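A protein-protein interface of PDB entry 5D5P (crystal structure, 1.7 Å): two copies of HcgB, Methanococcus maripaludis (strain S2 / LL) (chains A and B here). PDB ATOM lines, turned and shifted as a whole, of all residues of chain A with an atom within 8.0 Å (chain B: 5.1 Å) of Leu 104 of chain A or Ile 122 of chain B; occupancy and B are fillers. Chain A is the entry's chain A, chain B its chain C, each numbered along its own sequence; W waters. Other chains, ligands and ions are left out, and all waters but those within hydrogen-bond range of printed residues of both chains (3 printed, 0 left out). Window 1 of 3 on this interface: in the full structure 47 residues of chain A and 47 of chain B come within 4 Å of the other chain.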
ATOM      1  N   ASP A  76       7.824   5.791  23.553  1.00  0.00           N
ATOM      2  CA  ASP A  76       7.556   6.865  24.497  1.00  0.00           C
ATOM      3  C   ASP A  76       8.730   7.835  24.580  1.00  0.00           C
ATOM      4  O   ASP A  76       8.665   8.820  25.304  1.00  0.00           O
ATOM      5  CB  ASP A  76       7.237   6.271  25.871  1.00  0.00           C
ATOM      6  CG  ASP A  76       5.791   5.734  25.938  1.00  0.00           C
ATOM      7  OD1 ASP A  76       5.002   6.019  25.019  1.00  0.00           O
ATOM      8  OD2 ASP A  76       5.463   4.973  26.860  1.00  0.00           O
ATOM      9  N   THR A  78       9.749   9.268  21.804  1.00  0.00           N
ATOM     10  CA  THR A  78       9.612   9.971  20.523  1.00  0.00           C
ATOM     11  C   THR A  78       8.568  11.080  20.636  1.00  0.00           C
ATOM     12  O   THR A  78       7.802  11.154  21.619  1.00  0.00           O
ATOM     13  CB  THR A  78       9.190   9.058  19.341  1.00  0.00           C
ATOM     14  OG1 THR A  78       7.824   8.677  19.497  1.00  0.00           O
ATOM     15  CG2 THR A  78      10.066   7.814  19.228  1.00  0.00           C
ATOM     16  N   ARG A  79       8.535  11.938  19.629  1.00  0.00           N
ATOM     17  CA  ARG A  79       7.640  13.081  19.652  1.00  0.00           C
ATOM     18  C   ARG A  79       6.180  12.669  19.576  1.00  0.00           C
ATOM     19  O   ARG A  79       5.304  13.329  20.180  1.00  0.00           O
ATOM     20  CB  ARG A  79       7.983  14.038  18.503  1.00  0.00           C
ATOM     21  CG  ARG A  79       9.257  14.778  18.794  1.00  0.00           C
ATOM     22  CD  ARG A  79       9.347  16.070  18.001  1.00  0.00           C
ATOM     23  NE  ARG A  79      10.327  17.002  18.548  1.00  0.00           N
ATOM     24  CZ  ARG A  79      10.511  18.219  18.059  1.00  0.00           C
ATOM     25  NH1 ARG A  79       9.747  18.628  17.043  1.00  0.00           N
ATOM     26  NH2 ARG A  79      11.413  19.033  18.592  1.00  0.00           N
ATOM     27  N   MET A  80       5.907  11.567  18.881  1.00  0.00           N
ATOM     28  CA  MET A  80       4.529  11.114  18.712  1.00  0.00           C
ATOM     29  C   MET A  80       4.411   9.623  19.022  1.00  0.00           C
ATOM     30  O   MET A  80       4.455   8.778  18.107  1.00  0.00           O
ATOM     31  CB  MET A  80       4.049  11.450  17.293  1.00  0.00           C
ATOM     32  CG  MET A  80       3.837  12.941  17.147  1.00  0.00           C
ATOM     33  SD  MET A  80       3.118  13.294  15.556  1.00  0.00           S
ATOM     34  CE  MET A  80       4.613  12.954  14.684  1.00  0.00           C
ATOM     35  N   PRO A  81       4.303   9.292  20.323  1.00  0.00           N
ATOM     36  CA  PRO A  81       4.405   7.881  20.683  1.00  0.00           C
ATOM     37  C   PRO A  81       3.324   7.012  20.028  1.00  0.00           C
ATOM     38  O   PRO A  81       3.701   5.968  19.476  1.00  0.00           O
ATOM     39  CB  PRO A  81       4.288   7.905  22.208  1.00  0.00           C
ATOM     40  CG  PRO A  81       4.972   9.258  22.561  1.00  0.00           C
ATOM     41  CD  PRO A  81       4.374  10.162  21.516  1.00  0.00           C
ATOM     42  N   ALA A  82       2.047   7.421  20.057  1.00  0.00           N
ATOM     43  CA  ALA A  82       1.013   6.592  19.419  1.00  0.00           C
ATOM     44  C   ALA A  82       1.394   6.263  17.975  1.00  0.00           C
ATOM     45  O   ALA A  82       1.310   5.111  17.550  1.00  0.00           O
ATOM     46  CB  ALA A  82      -0.355   7.317  19.443  1.00  0.00           C
ATOM     47  N   LEU A  83       1.842   7.270  17.237  1.00  0.00           N
ATOM     48  CA  LEU A  83       2.179   7.072  15.839  1.00  0.00           C
ATOM     49  C   LEU A  83       3.333   6.077  15.704  1.00  0.00           C
ATOM     50  O   LEU A  83       3.289   5.147  14.894  1.00  0.00           O
ATOM     51  CB  LEU A  83       2.545   8.399  15.174  1.00  0.00           C
ATOM     52  CG  LEU A  83       3.080   8.249  13.746  1.00  0.00           C
ATOM     53  CD1 LEU A  83       1.979   7.852  12.757  1.00  0.00           C
ATOM     54  CD2 LEU A  83       3.775   9.529  13.288  1.00  0.00           C
ATOM     55  N   ARG A 101      -2.532   2.919  20.053  1.00  0.00           N
ATOM     56  CA  ARG A 101      -2.936   3.926  20.998  1.00  0.00           C
ATOM     57  C   ARG A 101      -1.731   4.242  21.852  1.00  0.00           C
ATOM     58  O   ARG A 101      -0.947   3.351  22.137  1.00  0.00           O
ATOM     59  CB  ARG A 101      -4.088   3.415  21.849  1.00  0.00           C
ATOM     60  CG  ARG A 101      -4.525   4.356  22.892  1.00  0.00           C
ATOM     61  CD  ARG A 101      -5.351   3.691  23.955  1.00  0.00           C
ATOM     62  NE  ARG A 101      -5.936   4.750  24.747  1.00  0.00           N
ATOM     63  CZ  ARG A 101      -5.635   5.018  26.006  1.00  0.00           C
ATOM     64  NH1 ARG A 101      -4.714   4.308  26.654  1.00  0.00           N
ATOM     65  NH2 ARG A 101      -6.265   6.016  26.597  1.00  0.00           N
ATOM     66  N   GLY A 102      -1.549   5.506  22.201  1.00  0.00           N
ATOM     67  CA  GLY A 102      -0.434   5.886  23.043  1.00  0.00           C
ATOM     68  C   GLY A 102      -0.502   7.378  23.252  1.00  0.00           C
ATOM     69  O   GLY A 102      -1.497   8.023  22.917  1.00  0.00           O
ATOM     70  N   ARG A 103       0.579   7.954  23.751  1.00  0.00           N
ATOM     71  CA  ARG A 103       0.584   9.386  24.000  1.00  0.00           C
ATOM     72  C   ARG A 103       0.457  10.158  22.684  1.00  0.00           C
ATOM     73  O   ARG A 103       0.958   9.720  21.656  1.00  0.00           O
ATOM     74  CB  ARG A 103       1.870   9.752  24.744  1.00  0.00           C
ATOM     75  CG  ARG A 103       1.754  10.919  25.616  1.00  0.00           C
ATOM     76  CD  ARG A 103       2.862  10.839  26.638  1.00  0.00           C
ATOM     77  NE  ARG A 103       4.161  11.025  25.996  1.00  0.00           N
ATOM     78  CZ  ARG A 103       5.288  10.388  26.331  1.00  0.00           C
ATOM     79  NH1 ARG A 103       5.314   9.489  27.315  1.00  0.00           N
ATOM     80  NH2 ARG A 103       6.425  10.688  25.685  1.00  0.00           N
ATOM     81  N   LEU A 104      -0.267  11.270  22.716  1.00  0.00           N
ATOM     82  CA  LEU A 104      -0.396  12.144  21.564  1.00  0.00           C
ATOM     83  C   LEU A 104       0.934  12.842  21.261  1.00  0.00           C
ATOM     84  O   LEU A 104       1.414  12.845  20.120  1.00  0.00           O
ATOM     85  CB  LEU A 104      -1.479  13.190  21.833  1.00  0.00           C
ATOM     86  CG  LEU A 104      -1.486  14.367  20.862  1.00  0.00           C
ATOM     87  CD1 LEU A 104      -1.831  13.918  19.412  1.00  0.00           C
ATOM     88  CD2 LEU A 104      -2.493  15.386  21.380  1.00  0.00           C
ATOM     89  N   GLY A 105       1.513  13.458  22.293  1.00  0.00           N
ATOM     90  CA  GLY A 105       2.730  14.246  22.101  1.00  0.00           C
ATOM     91  C   GLY A 105       3.579  14.078  23.350  1.00  0.00           C
ATOM     92  O   GLY A 105       3.893  12.957  23.715  1.00  0.00           O
ATOM     93  N   ILE A 106       3.913  15.184  24.011  1.00  0.00           N
ATOM     94  CA  ILE A 106       4.751  15.157  25.209  1.00  0.00           C
ATOM     95  C   ILE A 106       4.009  14.574  26.424  1.00  0.00           C
ATOM     96  O   ILE A 106       2.797  14.388  26.385  1.00  0.00           O
ATOM     97  CB  ILE A 106       5.265  16.567  25.554  1.00  0.00           C
ATOM     98  CG1 ILE A 106       4.123  17.436  26.106  1.00  0.00           C
ATOM     99  CG2 ILE A 106       5.945  17.216  24.324  1.00  0.00           C
ATOM    100  CD1 ILE A 106       4.661  18.696  26.852  1.00  0.00           C
ATOM    101  N   PRO A 107       4.749  14.245  27.499  1.00  0.00           N
ATOM    102  CA  PRO A 107       4.077  13.782  28.731  1.00  0.00           C
ATOM    103  C   PRO A 107       3.003  14.769  29.225  1.00  0.00           C
ATOM    104  O   PRO A 107       3.289  15.951  29.370  1.00  0.00           O
ATOM    105  CB  PRO A 107       5.228  13.681  29.750  1.00  0.00           C
ATOM    106  CG  PRO A 107       6.419  13.382  28.884  1.00  0.00           C
ATOM    107  CD  PRO A 107       6.223  14.164  27.611  1.00  0.00           C
ATOM    108  N   GLY A 108       1.795  14.274  29.479  1.00  0.00           N
ATOM    109  CA  GLY A 108       0.696  15.123  29.914  1.00  0.00           C
ATOM    110  C   GLY A 108      -0.258  15.467  28.782  1.00  0.00           C
ATOM    111  O   GLY A 108      -1.363  15.961  29.042  1.00  0.00           O
ATOM    112  N   SER A 109       0.138  15.184  27.536  1.00  0.00           N
ATOM    113  CA  SER A 109      -0.679  15.555  26.380  1.00  0.00           C
ATOM    114  C   SER A 109      -1.834  14.609  26.126  1.00  0.00           C
ATOM    115  O   SER A 109      -2.571  14.792  25.150  1.00  0.00           O
ATOM    116  CB  SER A 109       0.171  15.623  25.102  1.00  0.00           C
ATOM    117  OG  SER A 109       0.740  14.360  24.808  1.00  0.00           O
ATOM    118  N   GLY A 110      -2.003  13.604  26.987  1.00  0.00           N
ATOM    119  CA  GLY A 110      -3.120  12.671  26.844  1.00  0.00           C
ATOM    120  C   GLY A 110      -2.903  11.648  25.741  1.00  0.00           C
ATOM    121  O   GLY A 110      -1.777  11.522  25.212  1.00  0.00           O
ATOM    122  N   SER A 111      -3.978  10.959  25.357  1.00  0.00           N
ATOM    123  CA  SER A 111      -3.867   9.816  24.458  1.00  0.00           C
ATOM    124  C   SER A 111      -4.402  10.073  23.084  1.00  0.00           C
ATOM    125  O   SER A 111      -5.345  10.838  22.900  1.00  0.00           O
ATOM    126  CB  SER A 111      -4.613   8.605  25.029  1.00  0.00           C
ATOM    127  OG  SER A 111      -4.010   8.215  26.245  1.00  0.00           O
ATOM    128  N   LEU A 112      -3.789   9.375  22.128  1.00  0.00           N
ATOM    129  CA  LEU A 112      -4.232   9.383  20.733  1.00  0.00           C
ATOM    130  C   LEU A 112      -4.400   7.945  20.280  1.00  0.00           C
ATOM    131  O   LEU A 112      -3.503   7.114  20.520  1.00  0.00           O
ATOM    132  CB  LEU A 112      -3.187  10.108  19.841  1.00  0.00           C
ATOM    133  CG  LEU A 112      -3.403  10.012  18.340  1.00  0.00           C
ATOM    134  CD1 LEU A 112      -4.638  10.814  17.886  1.00  0.00           C
ATOM    135  CD2 LEU A 112      -2.140  10.504  17.605  1.00  0.00           C
ATOM    136  N   LEU A 113      -5.556   7.628  19.688  1.00  0.00           N
ATOM    137  CA  LEU A 113      -5.730   6.357  18.995  1.00  0.00           C
ATOM    138  C   LEU A 113      -5.714   6.637  17.482  1.00  0.00           C
ATOM    139  O   LEU A 113      -6.309   7.595  17.023  1.00  0.00           O
ATOM    140  CB  LEU A 113      -7.053   5.664  19.417  1.00  0.00           C
ATOM    141  CG  LEU A 113      -7.360   4.359  18.675  1.00  0.00           C
ATOM    142  CD1 LEU A 113      -8.134   3.420  19.605  1.00  0.00           C
ATOM    143  CD2 LEU A 113      -8.218   4.624  17.451  1.00  0.00           C
ATOM    144  N   LEU A 114      -5.015   5.793  16.722  1.00  0.00           N
ATOM    145  CA  LEU A 114      -4.973   5.891  15.264  1.00  0.00           C
ATOM    146  C   LEU A 114      -5.345   4.561  14.648  1.00  0.00           C
ATOM    147  O   LEU A 114      -5.044   3.488  15.190  1.00  0.00           O
ATOM    148  CB  LEU A 114      -3.574   6.281  14.766  1.00  0.00           C
ATOM    149  CG  LEU A 114      -3.029   7.645  15.224  1.00  0.00           C
ATOM    150  CD1 LEU A 114      -1.542   7.759  14.806  1.00  0.00           C
ATOM    151  CD2 LEU A 114      -3.833   8.775  14.613  1.00  0.00           C
ATOM    152  N   SER A 126      -8.668   9.401  17.269  1.00  0.00           N
ATOM    153  CA  SER A 126      -9.408  10.154  18.260  1.00  0.00           C
ATOM    154  C   SER A 126      -8.490  10.422  19.446  1.00  0.00           C
ATOM    155  O   SER A 126      -7.447   9.784  19.565  1.00  0.00           O
ATOM    156  CB  SER A 126     -10.624   9.365  18.700  1.00  0.00           C
ATOM    157  OG  SER A 126     -10.160   8.139  19.198  1.00  0.00           O
ATOM    158  N   VAL A 127      -8.856  11.368  20.298  1.00  0.00           N
ATOM    159  CA  VAL A 127      -7.992  11.684  21.439  1.00  0.00           C
ATOM    160  C   VAL A 127      -8.770  11.593  22.736  1.00  0.00           C
ATOM    161  O   VAL A 127      -9.987  11.666  22.736  1.00  0.00           O
ATOM    162  CB  VAL A 127      -7.337  13.083  21.323  1.00  0.00           C
ATOM    163  CG1 VAL A 127      -6.311  13.093  20.182  1.00  0.00           C
ATOM    164  CG2 VAL A 127      -8.384  14.167  21.170  1.00  0.00           C
ATOM    165  N   SER A 128      -8.068  11.387  23.850  1.00  0.00           N
ATOM    166  CA  SER A 128      -8.688  11.395  25.164  1.00  0.00           C
ATOM    167  C   SER A 128      -7.772  12.119  26.147  1.00  0.00           C
ATOM    168  O   SER A 128      -6.547  12.147  25.946  1.00  0.00           O
ATOM    169  CB  SER A 128      -8.962   9.948  25.618  1.00  0.00           C
ATOM    170  OG  SER A 128      -7.757   9.172  25.607  1.00  0.00           O
ATOM    171  N   LEU B  83       0.077  18.762  11.241  1.00  0.00           N
ATOM    172  CA  LEU B  83       1.364  18.797  11.913  1.00  0.00           C
ATOM    173  C   LEU B  83       2.384  19.588  11.111  1.00  0.00           C
ATOM    174  O   LEU B  83       3.055  20.456  11.616  1.00  0.00           O
ATOM    175  CB  LEU B  83       1.871  17.373  12.146  1.00  0.00           C
ATOM    176  CG  LEU B  83       3.296  17.347  12.663  1.00  0.00           C
ATOM    177  CD1 LEU B  83       3.364  17.863  14.096  1.00  0.00           C
ATOM    178  CD2 LEU B  83       3.882  15.928  12.522  1.00  0.00           C
ATOM    179  N   LEU B 114      -3.845  21.094  16.617  1.00  0.00           N
ATOM    180  CA  LEU B 114      -2.744  20.868  17.553  1.00  0.00           C
ATOM    181  C   LEU B 114      -2.315  22.177  18.172  1.00  0.00           C
ATOM    182  O   LEU B 114      -2.363  23.213  17.518  1.00  0.00           O
ATOM    183  CB  LEU B 114      -1.513  20.256  16.865  1.00  0.00           C
ATOM    184  CG  LEU B 114      -1.710  18.861  16.261  1.00  0.00           C
ATOM    185  CD1 LEU B 114      -0.483  18.538  15.388  1.00  0.00           C
ATOM    186  CD2 LEU B 114      -1.931  17.853  17.381  1.00  0.00           C
ATOM    187  N   ILE B 115      -1.894  22.100  19.434  1.00  0.00           N
ATOM    188  CA  ILE B 115      -1.149  23.199  20.047  1.00  0.00           C
ATOM    189  C   ILE B 115       0.275  22.707  20.233  1.00  0.00           C
ATOM    190  O   ILE B 115       0.497  21.712  20.915  1.00  0.00           O
ATOM    191  CB  ILE B 115      -1.746  23.660  21.383  1.00  0.00           C
ATOM    192  CG1 ILE B 115      -3.185  24.120  21.184  1.00  0.00           C
ATOM    193  CG2 ILE B 115      -0.923  24.818  21.964  1.00  0.00           C
ATOM    194  CD1 ILE B 115      -3.858  24.682  22.435  1.00  0.00           C
ATOM    195  N   MET B 116       1.206  23.394  19.568  1.00  0.00           N
ATOM    196  CA  MET B 116       2.613  23.026  19.553  1.00  0.00           C
ATOM    197  C   MET B 116       3.468  24.111  20.206  1.00  0.00           C
ATOM    198  O   MET B 116       3.100  25.281  20.226  1.00  0.00           O
ATOM    199  CB  MET B 116       3.070  22.777  18.108  1.00  0.00           C
ATOM    200  CG  MET B 116       2.315  21.600  17.498  1.00  0.00           C
ATOM    201  SD  MET B 116       2.410  21.544  15.686  1.00  0.00           S
ATOM    202  CE  MET B 116       4.160  21.425  15.470  1.00  0.00           C
ATOM    203  N   GLY B 120       8.214  22.629  18.224  1.00  0.00           N
ATOM    204  CA  GLY B 120       7.349  21.760  17.460  1.00  0.00           C
ATOM    205  C   GLY B 120       6.862  20.579  18.306  1.00  0.00           C
ATOM    206  O   GLY B 120       6.281  19.642  17.757  1.00  0.00           O
ATOM    207  N   ARG B 121       7.121  20.600  19.622  1.00  0.00           N
ATOM    208  CA  ARG B 121       6.569  19.530  20.470  1.00  0.00           C
ATOM    209  C   ARG B 121       5.064  19.675  20.613  1.00  0.00           C
ATOM    210  O   ARG B 121       4.548  20.790  20.677  1.00  0.00           O
ATOM    211  CB  ARG B 121       7.224  19.535  21.859  1.00  0.00           C
ATOM    212  CG  ARG B 121       8.749  19.233  21.763  1.00  0.00           C
ATOM    213  CD  ARG B 121       9.420  19.334  23.107  1.00  0.00           C
ATOM    214  NE  ARG B 121       9.450  20.719  23.548  1.00  0.00           N
ATOM    215  CZ  ARG B 121      10.317  21.219  24.422  1.00  0.00           C
ATOM    216  NH1 ARG B 121      11.254  20.445  24.971  1.00  0.00           N
ATOM    217  NH2 ARG B 121      10.252  22.514  24.745  1.00  0.00           N
ATOM    218  N   ILE B 122       4.352  18.551  20.677  1.00  0.00           N
ATOM    219  CA  ILE B 122       2.893  18.628  20.753  1.00  0.00           C
ATOM    220  C   ILE B 122       2.400  18.626  22.196  1.00  0.00           C
ATOM    221  O   ILE B 122       2.694  17.707  22.944  1.00  0.00           O
ATOM    222  CB  ILE B 122       2.286  17.447  19.995  1.00  0.00           C
ATOM    223  CG1 ILE B 122       2.634  17.591  18.505  1.00  0.00           C
ATOM    224  CG2 ILE B 122       0.788  17.367  20.216  1.00  0.00           C
ATOM    225  CD1 ILE B 122       2.441  16.316  17.722  1.00  0.00           C
ATOM    226  N   LEU B 123       1.636  19.664  22.574  1.00  0.00           N
ATOM    227  CA  LEU B 123       1.180  19.846  23.960  1.00  0.00           C
ATOM    228  C   LEU B 123      -0.222  19.303  24.139  1.00  0.00           C
ATOM    229  O   LEU B 123      -0.550  18.790  25.191  1.00  0.00           O
ATOM    230  CB  LEU B 123       1.165  21.317  24.367  1.00  0.00           C
ATOM    231  CG  LEU B 123       2.424  22.148  24.141  1.00  0.00           C
ATOM    232  CD1 LEU B 123       2.258  23.555  24.694  1.00  0.00           C
ATOM    233  CD2 LEU B 123       3.602  21.490  24.759  1.00  0.00           C
ATOM    234  N   THR B 124      -1.045  19.488  23.118  1.00  0.00           N
ATOM    235  CA  THR B 124      -2.432  19.020  23.208  1.00  0.00           C
ATOM    236  C   THR B 124      -3.062  19.120  21.836  1.00  0.00           C
ATOM    237  O   THR B 124      -2.443  19.629  20.882  1.00  0.00           O
ATOM    238  CB  THR B 124      -3.257  19.823  24.232  1.00  0.00           C
ATOM    239  OG1 THR B 124      -4.580  19.290  24.274  1.00  0.00           O
ATOM    240  CG2 THR B 124      -3.340  21.295  23.826  1.00  0.00           C
ATOM    241  N   GLY B 125      -4.279  18.598  21.699  1.00  0.00           N
ATOM    242  CA  GLY B 125      -4.890  18.599  20.383  1.00  0.00           C
ATOM    243  C   GLY B 125      -6.304  18.054  20.447  1.00  0.00           C
ATOM    244  O   GLY B 125      -6.752  17.654  21.490  1.00  0.00           O
ATOM    245  N   ARG B 152      -8.704  19.558  27.805  1.00  0.00           N
ATOM    246  CA  ARG B 152      -8.128  18.246  28.108  1.00  0.00           C
ATOM    247  C   ARG B 152      -6.754  18.359  28.754  1.00  0.00           C
ATOM    248  O   ARG B 152      -6.225  17.365  29.251  1.00  0.00           O
ATOM    249  CB  ARG B 152      -8.072  17.364  26.848  1.00  0.00           C
ATOM    250  CG  ARG B 152      -7.219  17.884  25.770  1.00  0.00           C
ATOM    251  CD  ARG B 152      -7.476  17.117  24.471  1.00  0.00           C
ATOM    252  NE  ARG B 152      -6.968  15.744  24.495  1.00  0.00           N
ATOM    253  CZ  ARG B 152      -5.668  15.433  24.438  1.00  0.00           C
ATOM    254  NH1 ARG B 152      -4.749  16.391  24.409  1.00  0.00           N
ATOM    255  NH2 ARG B 152      -5.293  14.148  24.448  1.00  0.00           N
HETATM  256  O   HOH W   1       5.942  16.074  20.743  1.00  0.00           O
HETATM  257  O   HOH W   2      -4.362  15.549  28.464  1.00  0.00           O
HETATM  258  O   HOH W   3       7.447  17.802  15.527  1.00  0.00           O
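The backbone NH of Ile 106 of chain A is in hydrogen-bond range of the backbone carbonyl oxygen of Ile 122 of chain B, 3.0 Å away.
NH1 of Arg 152 of chain B sits at hydrogen-bond distance from O of Ser 109 of chain A (2.8 Å).
O of Ser 128 of chain A lies within hydrogen-bond range of NH2 of Arg 152 of chain B, 2.8 Å away.
The guanidinium group of Arg 103 of chain A lies within hydrogen-bond range of the backbone carbonyl oxygen of Gly 105 of chain A (3.0 Å).
OG of Ser 109 of chain A lies within hydrogen-bond range of N of Gly 105 of chain A (2.8 Å).
O of Ile 106 of chain A sits at hydrogen-bond distance from OG of Ser 109 of chain A (2.6 Å).
The backbone NH of Ser 111 of chain A lies within hydrogen-bond range of the backbone carbonyl oxygen of Ser 128 of chain A (2.9 Å).
The backbone carbonyl oxygen (O) of Ile 115 of chain B sits at hydrogen-bond distance from the backbone NH (N) of Leu 123 of chain B, 2.9 Å away.
The backbone NH (N) of Ile 115 of chain B sits at hydrogen-bond distance from the backbone carbonyl oxygen (O) of Thr 124 of chain B (2.9 Å).
Among the printed residues, pairs that only touch across the chains: Arg 79 of chain A with Gly 120 of chain B, Met 80 of chain A with Leu 83 of chain B, Met 80 of chain A with Ile 122 of chain B, Leu 104 of chain A with Ile 122 of chain B, Leu 104 of chain A with Thr 124 of chain B, Leu 104 of chain A with Gly 125 of chain B, Leu 104 of chain A with Arg 152 of chain B, Gly 105 of chain A with Ile 122 of chain B, Ile 106 of chain A with Arg 121 of chain B, Ile 106 of chain A with Leu 123 of chain B, Ser 109 of chain A with Ile 122 of chain B, Ser 109 of chain A with Leu 123 of chain B, Gly 110 of chain A with Arg 152 of chain B, Ser 111 of chain A with Arg 152 of chain B, Val 127 of chain A with Gly 125 of chain B and Val 127 of chain A with Arg 152 of chain B.
Thr 78 of chain A touches none of the printed residues of chain B.
Leu 104 of chain A touches just these residues of chain B: Ile 122, Thr 124, Gly 125 and Arg 152.
Printed residues of chain B within 4 Å of Ser 109 of chain A: Ile 122, Leu 123 and Arg 152.
Printed residues of chain B within 4 Å of Gly 110 of chain A: Arg 152 (3.6 Å).
Of the printed residues of chain A, Gly 120 of chain B touches Arg 79.
Ile 122 of chain B touches just these residues of chain A: Met 80, Leu 104, Gly 105, Ile 106 and Ser 109.
Printed residues of chain A within 4 Å of Arg 152 of chain B: Leu 104, Ser 109, Gly 110, Ser 111, Val 127 and Ser 128.
The nearest residue of chain B that does not touch Leu 104 of chain A is Leu 114 of chain B (4.4 Å).
The nearest residue of chain A that does not touch Ile 122 of chain B is Arg 79 of chain A (4.8 Å).
The nearest printed residue of chain B that does not touch Gly 110 of chain A is Leu 123 of chain B (5.7 Å).
Printed residues of chain B that touch a printed residue of chain A: Leu 83, Gly 120, Arg 121, Ile 122, Leu 123, Thr 124, Gly 125 and Arg 152.
Hydrophobic or aromatic side chains of chain B within 4 Å of the printed part of chain A: Leu 83, Ile 122 and Leu 123.
Printed residues of chain A that touch a printed residue of chain B: Arg 79, Met 80, Leu 104, Gly 105, Ile 106, Ser 109, Gly 110, Ser 111, Val 127 and Ser 128.
2 positions are printed for both chains.
Of the 19 pairs that touch across the chains among the printed residues, none has its exchanged pair printed and touching as well.
Water W2 lies within hydrogen-bond range of the backbone carbonyl oxygen of Arg 152 of chain B (2.7 Å), the backbone carbonyl oxygen of Gly 108 of chain A (3.1 Å) and the backbone NH of Gly 110 of chain A (3.4 Å).
Water W1 bridges O of Arg 79 of chain A (2.9 Å) and N of Ile 122 of chain B (2.9 Å).
Water W3 bridges NH1 of Arg 79 of chain A (2.9 Å) and O of Gly 120 of chain B (3.1 Å).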
